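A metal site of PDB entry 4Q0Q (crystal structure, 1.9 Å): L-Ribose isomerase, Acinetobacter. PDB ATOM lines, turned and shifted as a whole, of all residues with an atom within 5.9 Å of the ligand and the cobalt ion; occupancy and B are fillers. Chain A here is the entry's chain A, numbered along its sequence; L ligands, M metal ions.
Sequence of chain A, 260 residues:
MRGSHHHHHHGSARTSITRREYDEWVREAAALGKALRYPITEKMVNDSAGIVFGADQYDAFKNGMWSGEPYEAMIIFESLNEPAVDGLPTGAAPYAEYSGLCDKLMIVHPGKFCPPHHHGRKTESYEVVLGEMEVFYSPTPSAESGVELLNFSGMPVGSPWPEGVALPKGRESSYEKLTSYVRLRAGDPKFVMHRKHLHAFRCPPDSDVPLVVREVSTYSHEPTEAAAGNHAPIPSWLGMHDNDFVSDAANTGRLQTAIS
The cobalt ion is bound by OE2 of Glu 124 (2.1 Å), NE2 of His 199 (2.2 Å), NE2 of His 119 (2.2 Å), O2 of the ligand (2.3 Å), O1 of the ligand (2.3 Å) and NE2 of His 117 (2.3 Å).
Within 4 Å of the cobalt ion: His 117, His 119, Glu 124 and His 199. Along chain A the residues within 4 Å of the cobalt ion span positions 117 to 199.
OE2 of Glu 215 lies within hydrogen-bond range of O3 of the ligand (3.3 Å). An oxygen (O4) of the ligand lies within hydrogen-bond range of the side-chain carboxylate (OE2) of Glu 222 (2.7 Å). NZ of Lys 122 sits at hydrogen-bond distance from O3 of the ligand, at 3.1 Å. The side-chain sulfur (SG) of Cys 114 is in hydrogen-bond range of an oxygen (O5) of the ligand, at 3.4 Å.
A ring nitrogen (ND1) of His 119 sits close to the side-chain amide oxygen of Asn 243 (3.1 Å). The side-chain carboxylate (OE1) of Glu 124 sits at hydrogen-bond distance from the side-chain hydroxyl (OH) of Tyr 126 (2.6 Å). OE2 of Glu 124 sits close to NZ of Lys 122, 3.8 Å away. OE1 of Glu 222 lies within hydrogen-bond range of OG of Ser 220, at 2.7 Å. SD of Met 74 sits at hydrogen-bond distance from SG of Cys 114 (3.6 Å). The side-chain amino group (NZ) of Lys 122 lies within salt-bridge range of the side-chain carboxylate (OE2) of Glu 215 (3.7 Å). N of Cys 114 sits at hydrogen-bond distance from O of Phe 201. The side-chain carboxylate (OE2) of Glu 222 lies within hydrogen-bond range of the side-chain amide nitrogen (ND2) of Asn 243, 2.7 Å away.
Ile 76 touches the ligand (CD1 to C4, 3.6 Å). CD of Lys 104 touches O3 of the ligand, at 3.9 Å. SD of Met 106 touches C1 of the ligand (3.9 Å). Phe 201 touches the ligand (CE2 to O1, 3.8 Å). NH1 of Arg 254 touches O4 of the ligand (3.6 Å). Hydrophobic or aromatic side chains within 4 Å of the ligand: Ile 76, Met 106, His 117, His 119, His 199 and Phe 201. Of the 20 residues printed, 13 come within 4 Å of the ligand. The nearest printed residue that does not touch the ligand is Tyr 126 (4.1 Å).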
ATOM      1  N   ILE A  51      17.018  13.309   2.881  1.00  0.00           N
ATOM      2  CA  ILE A  51      16.685  13.058   1.491  1.00  0.00           C
ATOM      3  C   ILE A  51      15.428  12.210   1.312  1.00  0.00           C
ATOM      4  O   ILE A  51      15.297  11.143   1.904  1.00  0.00           O
ATOM      5  CB  ILE A  51      17.846  12.333   0.791  1.00  0.00           C
ATOM      6  CG1 ILE A  51      19.135  13.134   0.986  1.00  0.00           C
ATOM      7  CG2 ILE A  51      17.542  12.162  -0.696  1.00  0.00           C
ATOM      8  CD1 ILE A  51      20.393  12.363   0.603  1.00  0.00           C
ATOM      9  N   PHE A  53      13.376  10.618  -1.850  1.00  0.00           N
ATOM     10  CA  PHE A  53      13.525  10.378  -3.291  1.00  0.00           C
ATOM     11  C   PHE A  53      12.249  10.426  -4.136  1.00  0.00           C
ATOM     12  O   PHE A  53      11.777   9.410  -4.643  1.00  0.00           O
ATOM     13  CB  PHE A  53      14.240   9.038  -3.521  1.00  0.00           C
ATOM     14  CG  PHE A  53      15.624   8.961  -2.886  1.00  0.00           C
ATOM     15  CD1 PHE A  53      15.775   8.564  -1.566  1.00  0.00           C
ATOM     16  CD2 PHE A  53      16.760   9.306  -3.625  1.00  0.00           C
ATOM     17  CE1 PHE A  53      17.052   8.492  -0.980  1.00  0.00           C
ATOM     18  CE2 PHE A  53      18.035   9.249  -3.048  1.00  0.00           C
ATOM     19  CZ  PHE A  53      18.176   8.832  -1.724  1.00  0.00           C
ATOM     20  N   MET A  74      16.179   8.892   3.343  1.00  0.00           N
ATOM     21  CA  MET A  74      17.319   8.615   4.208  1.00  0.00           C
ATOM     22  C   MET A  74      18.028   9.894   4.596  1.00  0.00           C
ATOM     23  O   MET A  74      17.765  10.965   4.046  1.00  0.00           O
ATOM     24  CB  MET A  74      18.317   7.724   3.482  1.00  0.00           C
ATOM     25  CG  MET A  74      19.152   8.482   2.452  1.00  0.00           C
ATOM     26  SD  MET A  74      20.039   7.418   1.301  1.00  0.00           S
ATOM     27  CE  MET A  74      21.339   6.786   2.372  1.00  0.00           C
ATOM     28  N   ILE A  76      21.883  11.646   5.248  1.00  0.00           N
ATOM     29  CA  ILE A  76      23.296  11.518   4.945  1.00  0.00           C
ATOM     30  C   ILE A  76      24.050  12.728   5.460  1.00  0.00           C
ATOM     31  O   ILE A  76      23.728  13.866   5.121  1.00  0.00           O
ATOM     32  CB  ILE A  76      23.556  11.401   3.421  1.00  0.00           C
ATOM     33  CG1 ILE A  76      22.892  10.136   2.868  1.00  0.00           C
ATOM     34  CG2 ILE A  76      25.055  11.397   3.154  1.00  0.00           C
ATOM     35  CD1 ILE A  76      23.029   9.958   1.366  1.00  0.00           C
ATOM     36  N   LYS A 104      30.927   9.633   4.703  1.00  0.00           N
ATOM     37  CA  LYS A 104      29.638  10.115   5.157  1.00  0.00           C
ATOM     38  C   LYS A 104      28.932   9.083   6.018  1.00  0.00           C
ATOM     39  O   LYS A 104      29.203   7.884   5.925  1.00  0.00           O
ATOM     40  CB  LYS A 104      28.749  10.484   3.966  1.00  0.00           C
ATOM     41  CG  LYS A 104      28.185   9.295   3.190  1.00  0.00           C
ATOM     42  CD  LYS A 104      28.671   9.289   1.738  1.00  0.00           C
ATOM     43  CE  LYS A 104      30.172   9.075   1.660  1.00  0.00           C
ATOM     44  NZ  LYS A 104      30.685   9.006   0.253  1.00  0.00           N
ATOM     45  N   MET A 106      25.355   7.440   6.965  1.00  0.00           N
ATOM     46  CA  MET A 106      24.023   7.287   6.396  1.00  0.00           C
ATOM     47  C   MET A 106      23.092   6.672   7.420  1.00  0.00           C
ATOM     48  O   MET A 106      23.438   5.695   8.086  1.00  0.00           O
ATOM     49  CB  MET A 106      24.095   6.423   5.129  1.00  0.00           C
ATOM     50  CG  MET A 106      25.050   6.995   4.076  1.00  0.00           C
ATOM     51  SD  MET A 106      25.026   6.139   2.466  1.00  0.00           S
ATOM     52  CE  MET A 106      25.711   4.563   2.933  1.00  0.00           C
ATOM     53  N   CYS A 114      17.465   3.195   0.483  1.00  0.00           N
ATOM     54  CA  CYS A 114      18.333   4.079  -0.263  1.00  0.00           C
ATOM     55  C   CYS A 114      18.007   3.316  -1.564  1.00  0.00           C
ATOM     56  O   CYS A 114      18.407   2.157  -1.734  1.00  0.00           O
ATOM     57  CB  CYS A 114      19.806   3.883   0.068  1.00  0.00           C
ATOM     58  SG  CYS A 114      20.871   4.842  -1.038  1.00  0.00           S
ATOM     59  N   HIS A 117      20.219   2.426  -7.842  1.00  0.00           N
ATOM     60  CA  HIS A 117      20.981   3.378  -8.629  1.00  0.00           C
ATOM     61  C   HIS A 117      22.381   2.829  -8.837  1.00  0.00           C
ATOM     62  O   HIS A 117      22.773   1.849  -8.219  1.00  0.00           O
ATOM     63  CB  HIS A 117      21.080   4.731  -7.914  1.00  0.00           C
ATOM     64  CG  HIS A 117      21.909   4.693  -6.661  1.00  0.00           C
ATOM     65  ND1 HIS A 117      21.454   4.147  -5.479  1.00  0.00           N
ATOM     66  CD2 HIS A 117      23.178   5.109  -6.413  1.00  0.00           C
ATOM     67  CE1 HIS A 117      22.405   4.236  -4.562  1.00  0.00           C
ATOM     68  NE2 HIS A 117      23.452   4.812  -5.101  1.00  0.00           N
ATOM     69  N   HIS A 119      26.630   4.208 -10.133  1.00  0.00           N
ATOM     70  CA  HIS A 119      27.512   5.332 -10.375  1.00  0.00           C
ATOM     71  C   HIS A 119      28.465   4.933 -11.495  1.00  0.00           C
ATOM     72  O   HIS A 119      28.932   3.799 -11.552  1.00  0.00           O
ATOM     73  CB  HIS A 119      28.313   5.661  -9.118  1.00  0.00           C
ATOM     74  CG  HIS A 119      27.471   5.880  -7.906  1.00  0.00           C
ATOM     75  ND1 HIS A 119      26.613   6.945  -7.772  1.00  0.00           N
ATOM     76  CD2 HIS A 119      27.351   5.164  -6.765  1.00  0.00           C
ATOM     77  CE1 HIS A 119      25.992   6.873  -6.613  1.00  0.00           C
ATOM     78  NE2 HIS A 119      26.421   5.809  -5.970  1.00  0.00           N
ATOM     79  N   LYS A 122      31.972   6.650  -9.240  1.00  0.00           N
ATOM     80  CA  LYS A 122      32.120   6.370  -7.821  1.00  0.00           C
ATOM     81  C   LYS A 122      32.037   4.928  -7.312  1.00  0.00           C
ATOM     82  O   LYS A 122      31.035   4.237  -7.519  1.00  0.00           O
ATOM     83  CB  LYS A 122      31.116   7.215  -7.029  1.00  0.00           C
ATOM     84  CG  LYS A 122      31.228   7.086  -5.508  1.00  0.00           C
ATOM     85  CD  LYS A 122      30.288   8.042  -4.775  1.00  0.00           C
ATOM     86  CE  LYS A 122      29.000   7.348  -4.347  1.00  0.00           C
ATOM     87  NZ  LYS A 122      28.031   8.310  -3.730  1.00  0.00           N
ATOM     88  N   GLU A 124      32.125   2.676  -3.827  1.00  0.00           N
ATOM     89  CA  GLU A 124      31.891   2.862  -2.401  1.00  0.00           C
ATOM     90  C   GLU A 124      32.137   1.608  -1.570  1.00  0.00           C
ATOM     91  O   GLU A 124      32.307   0.519  -2.103  1.00  0.00           O
ATOM     92  CB  GLU A 124      30.453   3.371  -2.158  1.00  0.00           C
ATOM     93  CG  GLU A 124      29.433   2.975  -3.233  1.00  0.00           C
ATOM     94  CD  GLU A 124      28.023   3.528  -2.985  1.00  0.00           C
ATOM     95  OE1 GLU A 124      27.278   2.964  -2.166  1.00  0.00           O
ATOM     96  OE2 GLU A 124      27.651   4.532  -3.636  1.00  0.00           O
ATOM     97  N   TYR A 126      31.055  -0.079   2.572  1.00  0.00           N
ATOM     98  CA  TYR A 126      30.171   0.073   3.718  1.00  0.00           C
ATOM     99  C   TYR A 126      30.711  -0.517   5.014  1.00  0.00           C
ATOM    100  O   TYR A 126      31.335  -1.571   5.033  1.00  0.00           O
ATOM    101  CB  TYR A 126      28.813  -0.576   3.442  1.00  0.00           C
ATOM    102  CG  TYR A 126      28.235  -0.284   2.085  1.00  0.00           C
ATOM    103  CD1 TYR A 126      28.139   1.026   1.613  1.00  0.00           C
ATOM    104  CD2 TYR A 126      27.794  -1.321   1.266  1.00  0.00           C
ATOM    105  CE1 TYR A 126      27.621   1.286   0.348  1.00  0.00           C
ATOM    106  CE2 TYR A 126      27.272  -1.070  -0.001  1.00  0.00           C
ATOM    107  CZ  TYR A 126      27.181   0.243  -0.450  1.00  0.00           C
ATOM    108  OH  TYR A 126      26.662   0.488  -1.695  1.00  0.00           O
ATOM    109  N   HIS A 199      22.881  -0.759  -7.165  1.00  0.00           N
ATOM    110  CA  HIS A 199      22.771  -1.098  -5.760  1.00  0.00           C
ATOM    111  C   HIS A 199      21.699  -0.302  -5.030  1.00  0.00           C
ATOM    112  O   HIS A 199      21.303   0.785  -5.454  1.00  0.00           O
ATOM    113  CB  HIS A 199      24.118  -0.948  -5.025  1.00  0.00           C
ATOM    114  CG  HIS A 199      24.665   0.453  -5.043  1.00  0.00           C
ATOM    115  ND1 HIS A 199      25.223   1.025  -6.163  1.00  0.00           N
ATOM    116  CD2 HIS A 199      24.746   1.390  -4.065  1.00  0.00           C
ATOM    117  CE1 HIS A 199      25.626   2.250  -5.879  1.00  0.00           C
ATOM    118  NE2 HIS A 199      25.341   2.493  -4.615  1.00  0.00           N
ATOM    119  N   PHE A 201      19.722  -0.390  -0.712  1.00  0.00           N
ATOM    120  CA  PHE A 201      19.757  -0.986   0.607  1.00  0.00           C
ATOM    121  C   PHE A 201      18.676  -0.426   1.519  1.00  0.00           C
ATOM    122  O   PHE A 201      18.141   0.652   1.278  1.00  0.00           O
ATOM    123  CB  PHE A 201      21.158  -0.830   1.244  1.00  0.00           C
ATOM    124  CG  PHE A 201      21.608   0.597   1.430  1.00  0.00           C
ATOM    125  CD1 PHE A 201      21.289   1.302   2.589  1.00  0.00           C
ATOM    126  CD2 PHE A 201      22.425   1.212   0.483  1.00  0.00           C
ATOM    127  CE1 PHE A 201      21.765   2.595   2.800  1.00  0.00           C
ATOM    128  CE2 PHE A 201      22.913   2.503   0.687  1.00  0.00           C
ATOM    129  CZ  PHE A 201      22.579   3.200   1.851  1.00  0.00           C
ATOM    130  N   GLU A 215      29.905   5.252   4.965  1.00  0.00           N
ATOM    131  CA  GLU A 215      30.343   4.965   3.621  1.00  0.00           C
ATOM    132  C   GLU A 215      31.676   5.655   3.370  1.00  0.00           C
ATOM    133  O   GLU A 215      31.835   6.835   3.689  1.00  0.00           O
ATOM    134  CB  GLU A 215      29.331   5.456   2.593  1.00  0.00           C
ATOM    135  CG  GLU A 215      29.809   5.285   1.161  1.00  0.00           C
ATOM    136  CD  GLU A 215      28.840   5.842   0.157  1.00  0.00           C
ATOM    137  OE1 GLU A 215      27.748   5.253   0.015  1.00  0.00           O
ATOM    138  OE2 GLU A 215      29.171   6.855  -0.498  1.00  0.00           O
ATOM    139  N   SER A 220      32.130  12.134  -4.651  1.00  0.00           N
ATOM    140  CA  SER A 220      30.703  12.134  -4.958  1.00  0.00           C
ATOM    141  C   SER A 220      30.308  13.377  -5.758  1.00  0.00           C
ATOM    142  O   SER A 220      30.306  14.501  -5.247  1.00  0.00           O
ATOM    143  CB  SER A 220      29.911  12.062  -3.646  1.00  0.00           C
ATOM    144  OG  SER A 220      28.526  11.950  -3.908  1.00  0.00           O
ATOM    145  N   GLU A 222      27.627  15.292  -6.897  1.00  0.00           N
ATOM    146  CA  GLU A 222      26.198  15.503  -6.687  1.00  0.00           C
ATOM    147  C   GLU A 222      25.830  16.985  -6.551  1.00  0.00           C
ATOM    148  O   GLU A 222      26.062  17.596  -5.516  1.00  0.00           O
ATOM    149  CB  GLU A 222      25.743  14.773  -5.421  1.00  0.00           C
ATOM    150  CG  GLU A 222      25.995  13.267  -5.431  1.00  0.00           C
ATOM    151  CD  GLU A 222      25.585  12.598  -4.120  1.00  0.00           C
ATOM    152  OE1 GLU A 222      26.196  12.913  -3.072  1.00  0.00           O
ATOM    153  OE2 GLU A 222      24.667  11.758  -4.145  1.00  0.00           O
ATOM    154  N   ASN A 243      25.112  10.251 -10.350  1.00  0.00           N
ATOM    155  CA  ASN A 243      24.081   9.374  -9.799  1.00  0.00           C
ATOM    156  C   ASN A 243      23.086   9.049 -10.889  1.00  0.00           C
ATOM    157  O   ASN A 243      22.619   9.939 -11.609  1.00  0.00           O
ATOM    158  CB  ASN A 243      23.336  10.028  -8.638  1.00  0.00           C
ATOM    159  CG  ASN A 243      24.231  10.311  -7.461  1.00  0.00           C
ATOM    160  OD1 ASN A 243      25.286   9.693  -7.299  1.00  0.00           O
ATOM    161  ND2 ASN A 243      23.803  11.235  -6.602  1.00  0.00           N
ATOM    162  N   PHE A 245      19.676   7.000 -10.862  1.00  0.00           N
ATOM    163  CA  PHE A 245      18.650   6.221 -10.191  1.00  0.00           C
ATOM    164  C   PHE A 245      17.719   5.565 -11.214  1.00  0.00           C
ATOM    165  O   PHE A 245      17.328   6.192 -12.206  1.00  0.00           O
ATOM    166  CB  PHE A 245      17.853   7.132  -9.252  1.00  0.00           C
ATOM    167  CG  PHE A 245      18.618   7.560  -8.039  1.00  0.00           C
ATOM    168  CD1 PHE A 245      18.591   6.784  -6.872  1.00  0.00           C
ATOM    169  CD2 PHE A 245      19.418   8.702  -8.062  1.00  0.00           C
ATOM    170  CE1 PHE A 245      19.348   7.151  -5.755  1.00  0.00           C
ATOM    171  CE2 PHE A 245      20.170   9.074  -6.957  1.00  0.00           C
ATOM    172  CZ  PHE A 245      20.142   8.298  -5.790  1.00  0.00           C
ATOM    173  N   ARG A 254      16.555  13.455  -5.166  1.00  0.00           N
ATOM    174  CA  ARG A 254      17.855  13.404  -4.515  1.00  0.00           C
ATOM    175  C   ARG A 254      18.486  14.795  -4.344  1.00  0.00           C
ATOM    176  O   ARG A 254      19.078  15.086  -3.306  1.00  0.00           O
ATOM    177  CB  ARG A 254      18.805  12.519  -5.333  1.00  0.00           C
ATOM    178  CG  ARG A 254      20.004  11.939  -4.559  1.00  0.00           C
ATOM    179  CD  ARG A 254      20.866  13.016  -3.916  1.00  0.00           C
ATOM    180  NE  ARG A 254      22.016  12.467  -3.198  1.00  0.00           N
ATOM    181  CZ  ARG A 254      22.705  13.122  -2.273  1.00  0.00           C
ATOM    182  NH1 ARG A 254      23.738  12.556  -1.674  1.00  0.00           N
ATOM    183  NH2 ARG A 254      22.340  14.357  -1.931  1.00  0.00           N
HETATM  184  C1  LIG L   1      25.021   5.184  -1.288  1.00  0.00           C
HETATM  185  O1  LIG L   1      24.861   4.091  -2.185  1.00  0.00           O
HETATM  186  C2  LIG L   1      24.812   6.505  -2.002  1.00  0.00           C
HETATM  187  O2  LIG L   1      25.709   6.608  -3.101  1.00  0.00           O
HETATM  188  C3  LIG L   1      24.927   7.740  -1.136  1.00  0.00           C
HETATM  189  O3  LIG L   1      26.247   8.253  -1.179  1.00  0.00           O
HETATM  190  C4  LIG L   1      23.970   8.715  -1.828  1.00  0.00           C
HETATM  191  O4  LIG L   1      24.641   9.329  -2.924  1.00  0.00           O
HETATM  192  C5  LIG L   1      22.877   7.802  -2.373  1.00  0.00           C
HETATM  193  O5  LIG L   1      23.477   6.507  -2.532  1.00  0.00           O
HETATM  194 CO    CO M   1      25.622   4.640  -4.293  1.00  0.00          CO
